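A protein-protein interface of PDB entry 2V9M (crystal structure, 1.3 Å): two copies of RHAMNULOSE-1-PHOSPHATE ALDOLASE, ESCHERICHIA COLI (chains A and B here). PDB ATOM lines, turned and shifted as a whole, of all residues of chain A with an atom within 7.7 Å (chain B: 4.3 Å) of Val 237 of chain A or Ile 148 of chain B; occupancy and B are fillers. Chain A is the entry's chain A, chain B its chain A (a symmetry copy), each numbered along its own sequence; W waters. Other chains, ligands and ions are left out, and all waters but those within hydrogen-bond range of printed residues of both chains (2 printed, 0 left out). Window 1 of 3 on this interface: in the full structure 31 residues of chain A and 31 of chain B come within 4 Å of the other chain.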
ATOM      1  N   ASN A 146      26.515 -30.904   2.305  1.00  0.00           N
ATOM      2  CA  ASN A 146      26.248 -30.903   0.865  1.00  0.00           C
ATOM      3  C   ASN A 146      27.168 -31.864   0.140  1.00  0.00           C
ATOM      4  O   ASN A 146      26.720 -32.521  -0.813  1.00  0.00           O
ATOM      5  CB  ASN A 146      26.363 -29.477   0.287  1.00  0.00           C
ATOM      6  CG  ASN A 146      25.207 -28.650   0.821  1.00  0.00           C
ATOM      7  OD1 ASN A 146      24.062 -28.783   0.393  1.00  0.00           O
ATOM      8  ND2 ASN A 146      25.500 -27.806   1.823  1.00  0.00           N
ATOM      9  N   LEU A 150      25.781 -34.910  -2.245  1.00  0.00           N
ATOM     10  CA  LEU A 150      26.218 -35.123  -3.602  1.00  0.00           C
ATOM     11  C   LEU A 150      26.674 -36.545  -3.878  1.00  0.00           C
ATOM     12  O   LEU A 150      26.569 -36.993  -5.002  1.00  0.00           O
ATOM     13  CB  LEU A 150      27.311 -34.136  -4.013  1.00  0.00           C
ATOM     14  CG  LEU A 150      26.833 -32.676  -4.182  1.00  0.00           C
ATOM     15  CD1 LEU A 150      28.039 -31.812  -4.623  1.00  0.00           C
ATOM     16  CD2 LEU A 150      25.675 -32.522  -5.155  1.00  0.00           C
ATOM     17  N   GLU A 167      33.706 -26.686 -11.056  1.00  0.00           N
ATOM     18  CA  GLU A 167      32.743 -25.819 -11.732  1.00  0.00           C
ATOM     19  C   GLU A 167      31.885 -25.039 -10.770  1.00  0.00           C
ATOM     20  O   GLU A 167      31.422 -23.974 -11.183  1.00  0.00           O
ATOM     21  CB  GLU A 167      31.843 -26.675 -12.635  1.00  0.00           C
ATOM     22  CG  GLU A 167      32.568 -27.226 -13.875  1.00  0.00           C
ATOM     23  CD  GLU A 167      31.710 -28.041 -14.790  1.00  0.00           C
ATOM     24  OE1 GLU A 167      30.464 -27.957 -14.710  1.00  0.00           O
ATOM     25  OE2 GLU A 167      32.306 -28.783 -15.628  1.00  0.00           O
ATOM     26  N   GLY A 168      31.630 -25.528  -9.561  1.00  0.00           N
ATOM     27  CA  GLY A 168      30.689 -24.921  -8.634  1.00  0.00           C
ATOM     28  C   GLY A 168      31.168 -23.724  -7.841  1.00  0.00           C
ATOM     29  O   GLY A 168      30.383 -23.157  -7.093  1.00  0.00           O
ATOM     30  N   SER A 169      32.444 -23.335  -7.962  1.00  0.00           N
ATOM     31  CA  SER A 169      32.969 -22.052  -7.460  1.00  0.00           C
ATOM     32  C   SER A 169      34.335 -21.861  -8.110  1.00  0.00           C
ATOM     33  O   SER A 169      35.161 -22.767  -8.085  1.00  0.00           O
ATOM     34  CB  SER A 169      33.121 -21.987  -5.950  1.00  0.00           C
ATOM     35  OG  SER A 169      31.857 -21.872  -5.289  1.00  0.00           O
ATOM     36  N   THR A 170      34.526 -20.654  -8.672  1.00  0.00           N
ATOM     37  CA  THR A 170      35.727 -20.413  -9.498  1.00  0.00           C
ATOM     38  C   THR A 170      37.034 -20.745  -8.804  1.00  0.00           C
ATOM     39  O   THR A 170      37.953 -21.276  -9.418  1.00  0.00           O
ATOM     40  CB  THR A 170      35.709 -18.952  -9.993  1.00  0.00           C
ATOM     41  OG1 THR A 170      34.728 -18.805 -11.018  1.00  0.00           O
ATOM     42  CG2 THR A 170      37.041 -18.540 -10.585  1.00  0.00           C
ATOM     43  N   GLU A 171      37.135 -20.440  -7.508  1.00  0.00           N
ATOM     44  CA  GLU A 171      38.305 -20.651  -6.657  1.00  0.00           C
ATOM     45  C   GLU A 171      38.725 -22.109  -6.548  1.00  0.00           C
ATOM     46  O   GLU A 171      39.871 -22.392  -6.239  1.00  0.00           O
ATOM     47  CB  GLU A 171      38.053 -20.150  -5.219  1.00  0.00           C
ATOM     48  CG  GLU A 171      36.918 -20.901  -4.558  1.00  0.00           C
ATOM     49  CD  GLU A 171      36.199 -20.232  -3.428  1.00  0.00           C
ATOM     50  OE1 GLU A 171      36.600 -19.200  -2.928  1.00  0.00           O
ATOM     51  OE2 GLU A 171      35.180 -20.720  -2.998  1.00  0.00           O
ATOM     52  N   ALA A 231      35.354 -26.634  -0.609  1.00  0.00           N
ATOM     53  CA  ALA A 231      34.689 -27.755  -1.295  1.00  0.00           C
ATOM     54  C   ALA A 231      33.211 -27.839  -0.916  1.00  0.00           C
ATOM     55  O   ALA A 231      32.379 -28.118  -1.758  1.00  0.00           O
ATOM     56  CB  ALA A 231      35.432 -29.057  -0.970  1.00  0.00           C
ATOM     57  N   GLU A 232      32.912 -27.637   0.377  1.00  0.00           N
ATOM     58  CA  GLU A 232      31.548 -27.715   0.860  1.00  0.00           C
ATOM     59  C   GLU A 232      30.698 -26.561   0.346  1.00  0.00           C
ATOM     60  O   GLU A 232      29.507 -26.722   0.059  1.00  0.00           O
ATOM     61  CB  GLU A 232      31.551 -27.779   2.387  1.00  0.00           C
ATOM     62  CG  GLU A 232      30.170 -27.705   3.036  1.00  0.00           C
ATOM     63  CD  GLU A 232      29.231 -28.786   2.668  1.00  0.00           C
ATOM     64  OE1 GLU A 232      28.023 -28.608   3.013  1.00  0.00           O
ATOM     65  OE2 GLU A 232      29.597 -29.825   2.081  1.00  0.00           O
ATOM     66  N   LYS A 233      31.283 -25.362   0.198  1.00  0.00           N
ATOM     67  CA  LYS A 233      30.574 -24.235  -0.406  1.00  0.00           C
ATOM     68  C   LYS A 233      30.221 -24.513  -1.866  1.00  0.00           C
ATOM     69  O   LYS A 233      29.089 -24.262  -2.307  1.00  0.00           O
ATOM     70  CB  LYS A 233      31.446 -22.973  -0.281  1.00  0.00           C
ATOM     71  CG  LYS A 233      30.942 -21.766  -1.038  1.00  0.00           C
ATOM     72  CD  LYS A 233      29.596 -21.253  -0.562  1.00  0.00           C
ATOM     73  CE  LYS A 233      29.281 -19.883  -1.117  1.00  0.00           C
ATOM     74  NZ  LYS A 233      29.965 -18.765  -0.363  1.00  0.00           N
ATOM     75  N   SER A 234      31.202 -25.049  -2.604  1.00  0.00           N
ATOM     76  CA  SER A 234      30.899 -25.451  -3.972  1.00  0.00           C
ATOM     77  C   SER A 234      29.784 -26.488  -3.998  1.00  0.00           C
ATOM     78  O   SER A 234      28.835 -26.399  -4.807  1.00  0.00           O
ATOM     79  CB  SER A 234      32.158 -25.947  -4.613  1.00  0.00           C
ATOM     80  OG  SER A 234      31.876 -26.313  -5.960  1.00  0.00           O
ATOM     81  N   ALA A 235      29.896 -27.468  -3.111  1.00  0.00           N
ATOM     82  CA  ALA A 235      28.818 -28.466  -3.035  1.00  0.00           C
ATOM     83  C   ALA A 235      27.464 -27.846  -2.749  1.00  0.00           C
ATOM     84  O   ALA A 235      26.441 -28.264  -3.294  1.00  0.00           O
ATOM     85  CB  ALA A 235      29.179 -29.524  -2.018  1.00  0.00           C
ATOM     86  N   GLN A 236      27.437 -26.856  -1.846  1.00  0.00           N
ATOM     87  CA  GLN A 236      26.175 -26.174  -1.505  1.00  0.00           C
ATOM     88  C   GLN A 236      25.584 -25.489  -2.721  1.00  0.00           C
ATOM     89  O   GLN A 236      24.373 -25.559  -2.971  1.00  0.00           O
ATOM     90  CB  GLN A 236      26.446 -25.147  -0.393  1.00  0.00           C
ATOM     91  CG  GLN A 236      25.195 -24.430   0.065  1.00  0.00           C
ATOM     92  CD  GLN A 236      25.497 -23.328   1.068  1.00  0.00           C
ATOM     93  OE1 GLN A 236      26.629 -22.883   1.210  1.00  0.00           O
ATOM     94  NE2 GLN A 236      24.417 -22.887   1.676  1.00  0.00           N
ATOM     95  N   VAL A 237      26.421 -24.800  -3.494  1.00  0.00           N
ATOM     96  CA  VAL A 237      26.002 -24.184  -4.737  1.00  0.00           C
ATOM     97  C   VAL A 237      25.456 -25.249  -5.703  1.00  0.00           C
ATOM     98  O   VAL A 237      24.380 -25.119  -6.289  1.00  0.00           O
ATOM     99  CB  VAL A 237      27.175 -23.403  -5.362  1.00  0.00           C
ATOM    100  CG1 VAL A 237      26.907 -22.998  -6.810  1.00  0.00           C
ATOM    101  CG2 VAL A 237      27.527 -22.178  -4.514  1.00  0.00           C
ATOM    102  N   LEU A 238      26.189 -26.331  -5.872  1.00  0.00           N
ATOM    103  CA  LEU A 238      25.766 -27.400  -6.754  1.00  0.00           C
ATOM    104  C   LEU A 238      24.432 -28.007  -6.353  1.00  0.00           C
ATOM    105  O   LEU A 238      23.581 -28.257  -7.209  1.00  0.00           O
ATOM    106  CB  LEU A 238      26.830 -28.493  -6.846  1.00  0.00           C
ATOM    107  CG  LEU A 238      28.152 -28.134  -7.519  1.00  0.00           C
ATOM    108  CD1 LEU A 238      29.144 -29.287  -7.360  1.00  0.00           C
ATOM    109  CD2 LEU A 238      27.998 -27.769  -8.962  1.00  0.00           C
ATOM    110  N   VAL A 239      24.228 -28.254  -5.065  1.00  0.00           N
ATOM    111  CA  VAL A 239      22.939 -28.813  -4.646  1.00  0.00           C
ATOM    112  C   VAL A 239      21.812 -27.873  -5.028  1.00  0.00           C
ATOM    113  O   VAL A 239      20.752 -28.330  -5.512  1.00  0.00           O
ATOM    114  CB  VAL A 239      22.934 -29.111  -3.135  1.00  0.00           C
ATOM    115  CG1 VAL A 239      21.571 -29.425  -2.613  1.00  0.00           C
ATOM    116  CG2 VAL A 239      23.896 -30.257  -2.846  1.00  0.00           C
ATOM    117  N   LYS A 240      21.997 -26.557  -4.868  1.00  0.00           N
ATOM    118  CA  LYS A 240      20.982 -25.621  -5.319  1.00  0.00           C
ATOM    119  C   LYS A 240      20.773 -25.711  -6.832  1.00  0.00           C
ATOM    120  O   LYS A 240      19.614 -25.771  -7.302  1.00  0.00           O
ATOM    121  CB  LYS A 240      21.375 -24.192  -4.938  1.00  0.00           C
ATOM    122  CG  LYS A 240      21.283 -23.898  -3.427  1.00  0.00           C
ATOM    123  CD  LYS A 240      21.886 -22.553  -3.102  1.00  0.00           C
ATOM    124  CE  LYS A 240      21.829 -22.185  -1.618  1.00  0.00           C
ATOM    125  NZ  LYS A 240      20.488 -21.946  -1.122  1.00  0.00           N
ATOM    126  N   VAL A 241      21.863 -25.700  -7.584  1.00  0.00           N
ATOM    127  CA  VAL A 241      21.749 -25.768  -9.051  1.00  0.00           C
ATOM    128  C   VAL A 241      21.055 -27.044  -9.514  1.00  0.00           C
ATOM    129  O   VAL A 241      20.141 -26.993 -10.382  1.00  0.00           O
ATOM    130  CB  VAL A 241      23.151 -25.618  -9.694  1.00  0.00           C
ATOM    131  CG1 VAL A 241      23.070 -25.901 -11.204  1.00  0.00           C
ATOM    132  CG2 VAL A 241      23.695 -24.226  -9.405  1.00  0.00           C
ATOM    133  N   TYR A 242      21.434 -28.174  -8.988  1.00  0.00           N
ATOM    134  CA  TYR A 242      20.814 -29.430  -9.358  1.00  0.00           C
ATOM    135  C   TYR A 242      19.339 -29.447  -8.961  1.00  0.00           C
ATOM    136  O   TYR A 242      18.489 -29.917  -9.733  1.00  0.00           O
ATOM    137  CB  TYR A 242      21.570 -30.602  -8.743  1.00  0.00           C
ATOM    138  CG  TYR A 242      23.033 -30.767  -9.140  1.00  0.00           C
ATOM    139  CD1 TYR A 242      23.900 -31.428  -8.309  1.00  0.00           C
ATOM    140  CD2 TYR A 242      23.537 -30.251 -10.326  1.00  0.00           C
ATOM    141  CE1 TYR A 242      25.234 -31.617  -8.574  1.00  0.00           C
ATOM    142  CE2 TYR A 242      24.897 -30.418 -10.646  1.00  0.00           C
ATOM    143  CZ  TYR A 242      25.681 -31.109  -9.768  1.00  0.00           C
ATOM    144  OH  TYR A 242      27.027 -31.382  -9.848  1.00  0.00           O
ATOM    145  N   SER A 243      18.989 -28.880  -7.817  1.00  0.00           N
ATOM    146  CA  SER A 243      17.596 -28.780  -7.373  1.00  0.00           C
ATOM    147  C   SER A 243      16.735 -27.893  -8.251  1.00  0.00           C
ATOM    148  O   SER A 243      15.518 -28.039  -8.305  1.00  0.00           O
ATOM    149  CB  SER A 243      17.537 -28.286  -5.928  1.00  0.00           C
ATOM    150  OG  SER A 243      18.175 -29.204  -5.061  1.00  0.00           O
ATOM    151  N   MET A 244      17.368 -26.957  -8.953  1.00  0.00           N
ATOM    152  CA  MET A 244      16.734 -26.059  -9.924  1.00  0.00           C
ATOM    153  C   MET A 244      16.713 -26.627 -11.336  1.00  0.00           C
ATOM    154  O   MET A 244      16.318 -25.929 -12.265  1.00  0.00           O
ATOM    155  CB  MET A 244      17.388 -24.682  -9.918  1.00  0.00           C
ATOM    156  CG  MET A 244      17.242 -23.906  -8.627  1.00  0.00           C
ATOM    157  SD  MET A 244      17.852 -22.230  -8.728  1.00  0.00           S
ATOM    158  CE  MET A 244      19.629 -22.484  -8.689  1.00  0.00           C
ATOM    159  N   MET A 247      22.598 -27.313 -14.541  1.00  0.00           N
ATOM    160  CA  MET A 247      23.311 -26.231 -15.192  1.00  0.00           C
ATOM    161  C   MET A 247      22.848 -25.909 -16.591  1.00  0.00           C
ATOM    162  O   MET A 247      22.875 -26.762 -17.479  1.00  0.00           O
ATOM    163  CB  MET A 247      24.797 -26.647 -15.296  1.00  0.00           C
ATOM    164  CG  MET A 247      25.490 -26.744 -13.942  1.00  0.00           C
ATOM    165  SD  MET A 247      27.152 -27.400 -14.161  1.00  0.00           S
ATOM    166  CE  MET A 247      27.750 -27.312 -12.472  1.00  0.00           C
ATOM    167  N   HIS B 143      31.232 -13.914  -1.844  1.00  0.00           N
ATOM    168  CA  HIS B 143      30.782 -15.092  -2.590  1.00  0.00           C
ATOM    169  C   HIS B 143      29.338 -15.402  -2.145  1.00  0.00           C
ATOM    170  O   HIS B 143      29.064 -16.398  -1.494  1.00  0.00           O
ATOM    171  CB  HIS B 143      31.746 -16.250  -2.411  1.00  0.00           C
ATOM    172  CG  HIS B 143      33.099 -15.957  -2.983  1.00  0.00           C
ATOM    173  ND1 HIS B 143      34.130 -16.832  -2.848  1.00  0.00           N
ATOM    174  CD2 HIS B 143      33.621 -14.901  -3.684  1.00  0.00           C
ATOM    175  CE1 HIS B 143      35.219 -16.329  -3.449  1.00  0.00           C
ATOM    176  NE2 HIS B 143      34.925 -15.143  -3.985  1.00  0.00           N
ATOM    177  N   ALA B 144      28.419 -14.540  -2.475  1.00  0.00           N
ATOM    178  CA  ALA B 144      27.011 -14.615  -2.074  1.00  0.00           C
ATOM    179  C   ALA B 144      26.371 -15.850  -2.726  1.00  0.00           C
ATOM    180  O   ALA B 144      26.233 -15.914  -3.953  1.00  0.00           O
ATOM    181  CB  ALA B 144      26.271 -13.344  -2.437  1.00  0.00           C
ATOM    182  N   THR B 145      26.018 -16.816  -1.896  1.00  0.00           N
ATOM    183  CA  THR B 145      25.721 -18.167  -2.313  1.00  0.00           C
ATOM    184  C   THR B 145      24.613 -18.302  -3.354  1.00  0.00           C
ATOM    185  O   THR B 145      24.787 -19.005  -4.368  1.00  0.00           O
ATOM    186  CB  THR B 145      25.335 -18.993  -1.058  1.00  0.00           C
ATOM    187  OG1 THR B 145      26.343 -18.722  -0.058  1.00  0.00           O
ATOM    188  CG2 THR B 145      25.262 -20.476  -1.376  1.00  0.00           C
ATOM    189  N   ASN B 146      23.453 -17.723  -3.102  1.00  0.00           N
ATOM    190  CA  ASN B 146      22.319 -17.891  -4.013  1.00  0.00           C
ATOM    191  C   ASN B 146      22.533 -17.116  -5.298  1.00  0.00           C
ATOM    192  O   ASN B 146      22.153 -17.612  -6.370  1.00  0.00           O
ATOM    193  CB  ASN B 146      21.000 -17.482  -3.327  1.00  0.00           C
ATOM    194  CG  ASN B 146      20.686 -18.500  -2.247  1.00  0.00           C
ATOM    195  OD1 ASN B 146      20.255 -19.620  -2.515  1.00  0.00           O
ATOM    196  ND2 ASN B 146      20.959 -18.125  -0.987  1.00  0.00           N
ATOM    197  N   LEU B 147      23.142 -15.930  -5.224  1.00  0.00           N
ATOM    198  CA  LEU B 147      23.487 -15.225  -6.461  1.00  0.00           C
ATOM    199  C   LEU B 147      24.408 -16.076  -7.342  1.00  0.00           C
ATOM    200  O   LEU B 147      24.214 -16.138  -8.558  1.00  0.00           O
ATOM    201  CB  LEU B 147      24.117 -13.853  -6.174  1.00  0.00           C
ATOM    202  CG  LEU B 147      23.115 -12.798  -5.656  1.00  0.00           C
ATOM    203  CD1 LEU B 147      23.851 -11.639  -4.990  1.00  0.00           C
ATOM    204  CD2 LEU B 147      22.241 -12.299  -6.821  1.00  0.00           C
ATOM    205  N   ILE B 148      25.393 -16.721  -6.721  1.00  0.00           N
ATOM    206  CA  ILE B 148      26.272 -17.606  -7.464  1.00  0.00           C
ATOM    207  C   ILE B 148      25.470 -18.714  -8.089  1.00  0.00           C
ATOM    208  O   ILE B 148      25.598 -19.003  -9.289  1.00  0.00           O
ATOM    209  CB  ILE B 148      27.405 -18.172  -6.571  1.00  0.00           C
ATOM    210  CG1 ILE B 148      28.352 -17.082  -6.079  1.00  0.00           C
ATOM    211  CG2 ILE B 148      28.172 -19.274  -7.277  1.00  0.00           C
ATOM    212  CD1 ILE B 148      29.201 -17.508  -4.894  1.00  0.00           C
ATOM    213  N   ALA B 149      24.626 -19.414  -7.346  1.00  0.00           N
ATOM    214  CA  ALA B 149      23.852 -20.514  -7.914  1.00  0.00           C
ATOM    215  C   ALA B 149      23.030 -20.070  -9.101  1.00  0.00           C
ATOM    216  O   ALA B 149      22.911 -20.783 -10.108  1.00  0.00           O
ATOM    217  CB  ALA B 149      22.919 -21.095  -6.828  1.00  0.00           C
ATOM    218  N   LEU B 150      22.424 -18.873  -9.011  1.00  0.00           N
ATOM    219  CA  LEU B 150      21.606 -18.395 -10.096  1.00  0.00           C
ATOM    220  C   LEU B 150      22.374 -18.188 -11.390  1.00  0.00           C
ATOM    221  O   LEU B 150      21.789 -18.298 -12.450  1.00  0.00           O
ATOM    222  CB  LEU B 150      20.854 -17.117  -9.726  1.00  0.00           C
ATOM    223  CG  LEU B 150      19.723 -17.310  -8.691  1.00  0.00           C
ATOM    224  CD1 LEU B 150      19.044 -15.940  -8.443  1.00  0.00           C
ATOM    225  CD2 LEU B 150      18.696 -18.354  -9.098  1.00  0.00           C
ATOM    226  N   THR B 151      23.677 -17.916 -11.284  1.00  0.00           N
ATOM    227  CA  THR B 151      24.432 -17.724 -12.524  1.00  0.00           C
ATOM    228  C   THR B 151      24.599 -19.009 -13.329  1.00  0.00           C
ATOM    229  O   THR B 151      25.056 -18.944 -14.480  1.00  0.00           O
ATOM    230  CB  THR B 151      25.805 -17.049 -12.288  1.00  0.00           C
ATOM    231  OG1 THR B 151      26.571 -17.956 -11.502  1.00  0.00           O
ATOM    232  CG2 THR B 151      25.666 -15.708 -11.569  1.00  0.00           C
ATOM    233  N   TYR B 152      24.273 -20.155 -12.782  1.00  0.00           N
ATOM    234  CA  TYR B 152      24.292 -21.414 -13.530  1.00  0.00           C
ATOM    235  C   TYR B 152      22.950 -21.700 -14.214  1.00  0.00           C
ATOM    236  O   TYR B 152      22.877 -22.605 -15.055  1.00  0.00           O
ATOM    237  CB  TYR B 152      24.653 -22.640 -12.660  1.00  0.00           C
ATOM    238  CG  TYR B 152      26.016 -22.520 -12.024  1.00  0.00           C
ATOM    239  CD1 TYR B 152      26.222 -21.786 -10.853  1.00  0.00           C
ATOM    240  CD2 TYR B 152      27.138 -23.142 -12.570  1.00  0.00           C
ATOM    241  CE1 TYR B 152      27.452 -21.673 -10.289  1.00  0.00           C
ATOM    242  CE2 TYR B 152      28.367 -23.021 -12.005  1.00  0.00           C
ATOM    243  CZ  TYR B 152      28.521 -22.289 -10.850  1.00  0.00           C
ATOM    244  OH  TYR B 152      29.751 -22.132 -10.242  1.00  0.00           O
ATOM    245  N   HIS B 212      31.152 -17.212  -9.562  1.00  0.00           N
ATOM    246  CA  HIS B 212      32.158 -16.655  -8.645  1.00  0.00           C
ATOM    247  C   HIS B 212      31.459 -15.809  -7.591  1.00  0.00           C
ATOM    248  O   HIS B 212      31.613 -16.153  -6.406  1.00  0.00           O
ATOM    249  CB  HIS B 212      33.231 -15.890  -9.441  1.00  0.00           C
ATOM    250  CG  HIS B 212      34.352 -15.346  -8.607  1.00  0.00           C
ATOM    251  ND1 HIS B 212      35.557 -14.968  -9.118  1.00  0.00           N
ATOM    252  CD2 HIS B 212      34.525 -15.084  -7.270  1.00  0.00           C
ATOM    253  CE1 HIS B 212      36.340 -14.526  -8.154  1.00  0.00           C
ATOM    254  NE2 HIS B 212      35.739 -14.575  -6.985  1.00  0.00           N
ATOM    255  N   GLY B 213      30.900 -14.663  -7.867  1.00  0.00           N
ATOM    256  CA  GLY B 213      30.383 -13.848  -6.772  1.00  0.00           C
ATOM    257  C   GLY B 213      29.939 -12.484  -7.191  1.00  0.00           C
ATOM    258  O   GLY B 213      29.591 -12.281  -8.369  1.00  0.00           O
HETATM  259  O   HOH W   1      20.733 -20.208   1.237  1.00  0.00           O
HETATM  260  O   HOH W   2      17.372 -20.766  -1.303  1.00  0.00           O
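Positions printed for both chains: 146 and 150.
The backbone carbonyl oxygen (O) of Ile 148 of chain B lies within hydrogen-bond range of the side-chain hydroxyl (OG1) of Thr 151 of chain B, at 2.6 Å.
Water W1 lies within hydrogen-bond range of the side-chain amino group (NZ) of Lys 240 of chain A (2.9 Å) and the side-chain amide nitrogen (ND2) of Asn 146 of chain B (3.1 Å). Water W2 bridges the side-chain amide oxygen of Asn 146 of chain B (3.3 Å) and the side-chain amino group of Lys 240 of chain A (3.3 Å).
Among the printed residues, merely in contact across the chains: Ser 169 of chain A with Tyr 152 of chain B (3.7 Å), Thr 170 of chain A with His 212 of chain B (3.6 Å), Lys 233 of chain A with Thr 145 of chain B (3.3 Å), Gln 236 of chain A with Thr 145 of chain B (3.8 Å), Val 237 of chain A with Ile 148 of chain B (3.96 Å), Val 237 of chain A with Tyr 152 of chain B (3.8 Å), Lys 240 of chain A with Thr 145 of chain B (3.8 Å), Lys 240 of chain A with Ala 149 of chain B (3.9 Å), Val 241 of chain A with Ala 149 of chain B (3.6 Å), Val 241 of chain A with Tyr 152 of chain B (3.7 Å), Met 244 of chain A with Ala 149 of chain B (3.96 Å), Met 244 of chain A with Leu 150 of chain B (3.98 Å) and Met 247 of chain A with Tyr 152 of chain B (3.6 Å).
Ile 148 of chain B touches one residue of chain A. Of the printed residues of chain B, Thr 170 of chain A touches His 212. Of the printed residues of chain A, Asn 146 of chain B touches Lys 240. Of the printed residues of chain B, Glu 167 of chain A touches Tyr 152 (2.7 Å). Leu 150 of chain A touches none of the printed residues of chain B. Leu 147 of chain B touches none of the printed residues of chain A. The nearest residue of chain B that does not touch Val 237 of chain A is Ala 149 of chain B (4.1 Å). The nearest printed residue of chain A that does not touch Ile 148 of chain B is Lys 233 of chain A (4.5 Å). The nearest printed residue of chain B that does not touch Lys 240 of chain A is Leu 150 of chain B (6.8 Å).
Of the 12 printed residues of chain B, 8 touch a printed residue of chain A. Among the printed residues, 18 pairs touch across the chains. Among the printed residues, no Asp or Glu carboxylate lies within 4 Å of a Lys or Arg side-chain nitrogen of the other chain.
The side-chain hydroxyl (OH) of Tyr 152 of chain B lies within hydrogen-bond range of the backbone carbonyl oxygen (O) of Glu 167 of chain A. O of Gly 168 of chain A lies close to OH of Tyr 152 of chain B, at 3.4 Å. OE1 of Glu 171 of chain A sits close to ND1 of His 143 of chain B (3.4 Å). The backbone carbonyl oxygen (O) of His 143 of chain B lies within hydrogen-bond range of the side-chain amino group (NZ) of Lys 233 of chain A, 2.8 Å away. The side-chain amide oxygen (OD1) of Asn 146 of chain B sits at hydrogen-bond distance from the side-chain amino group (NZ) of Lys 240 of chain A.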
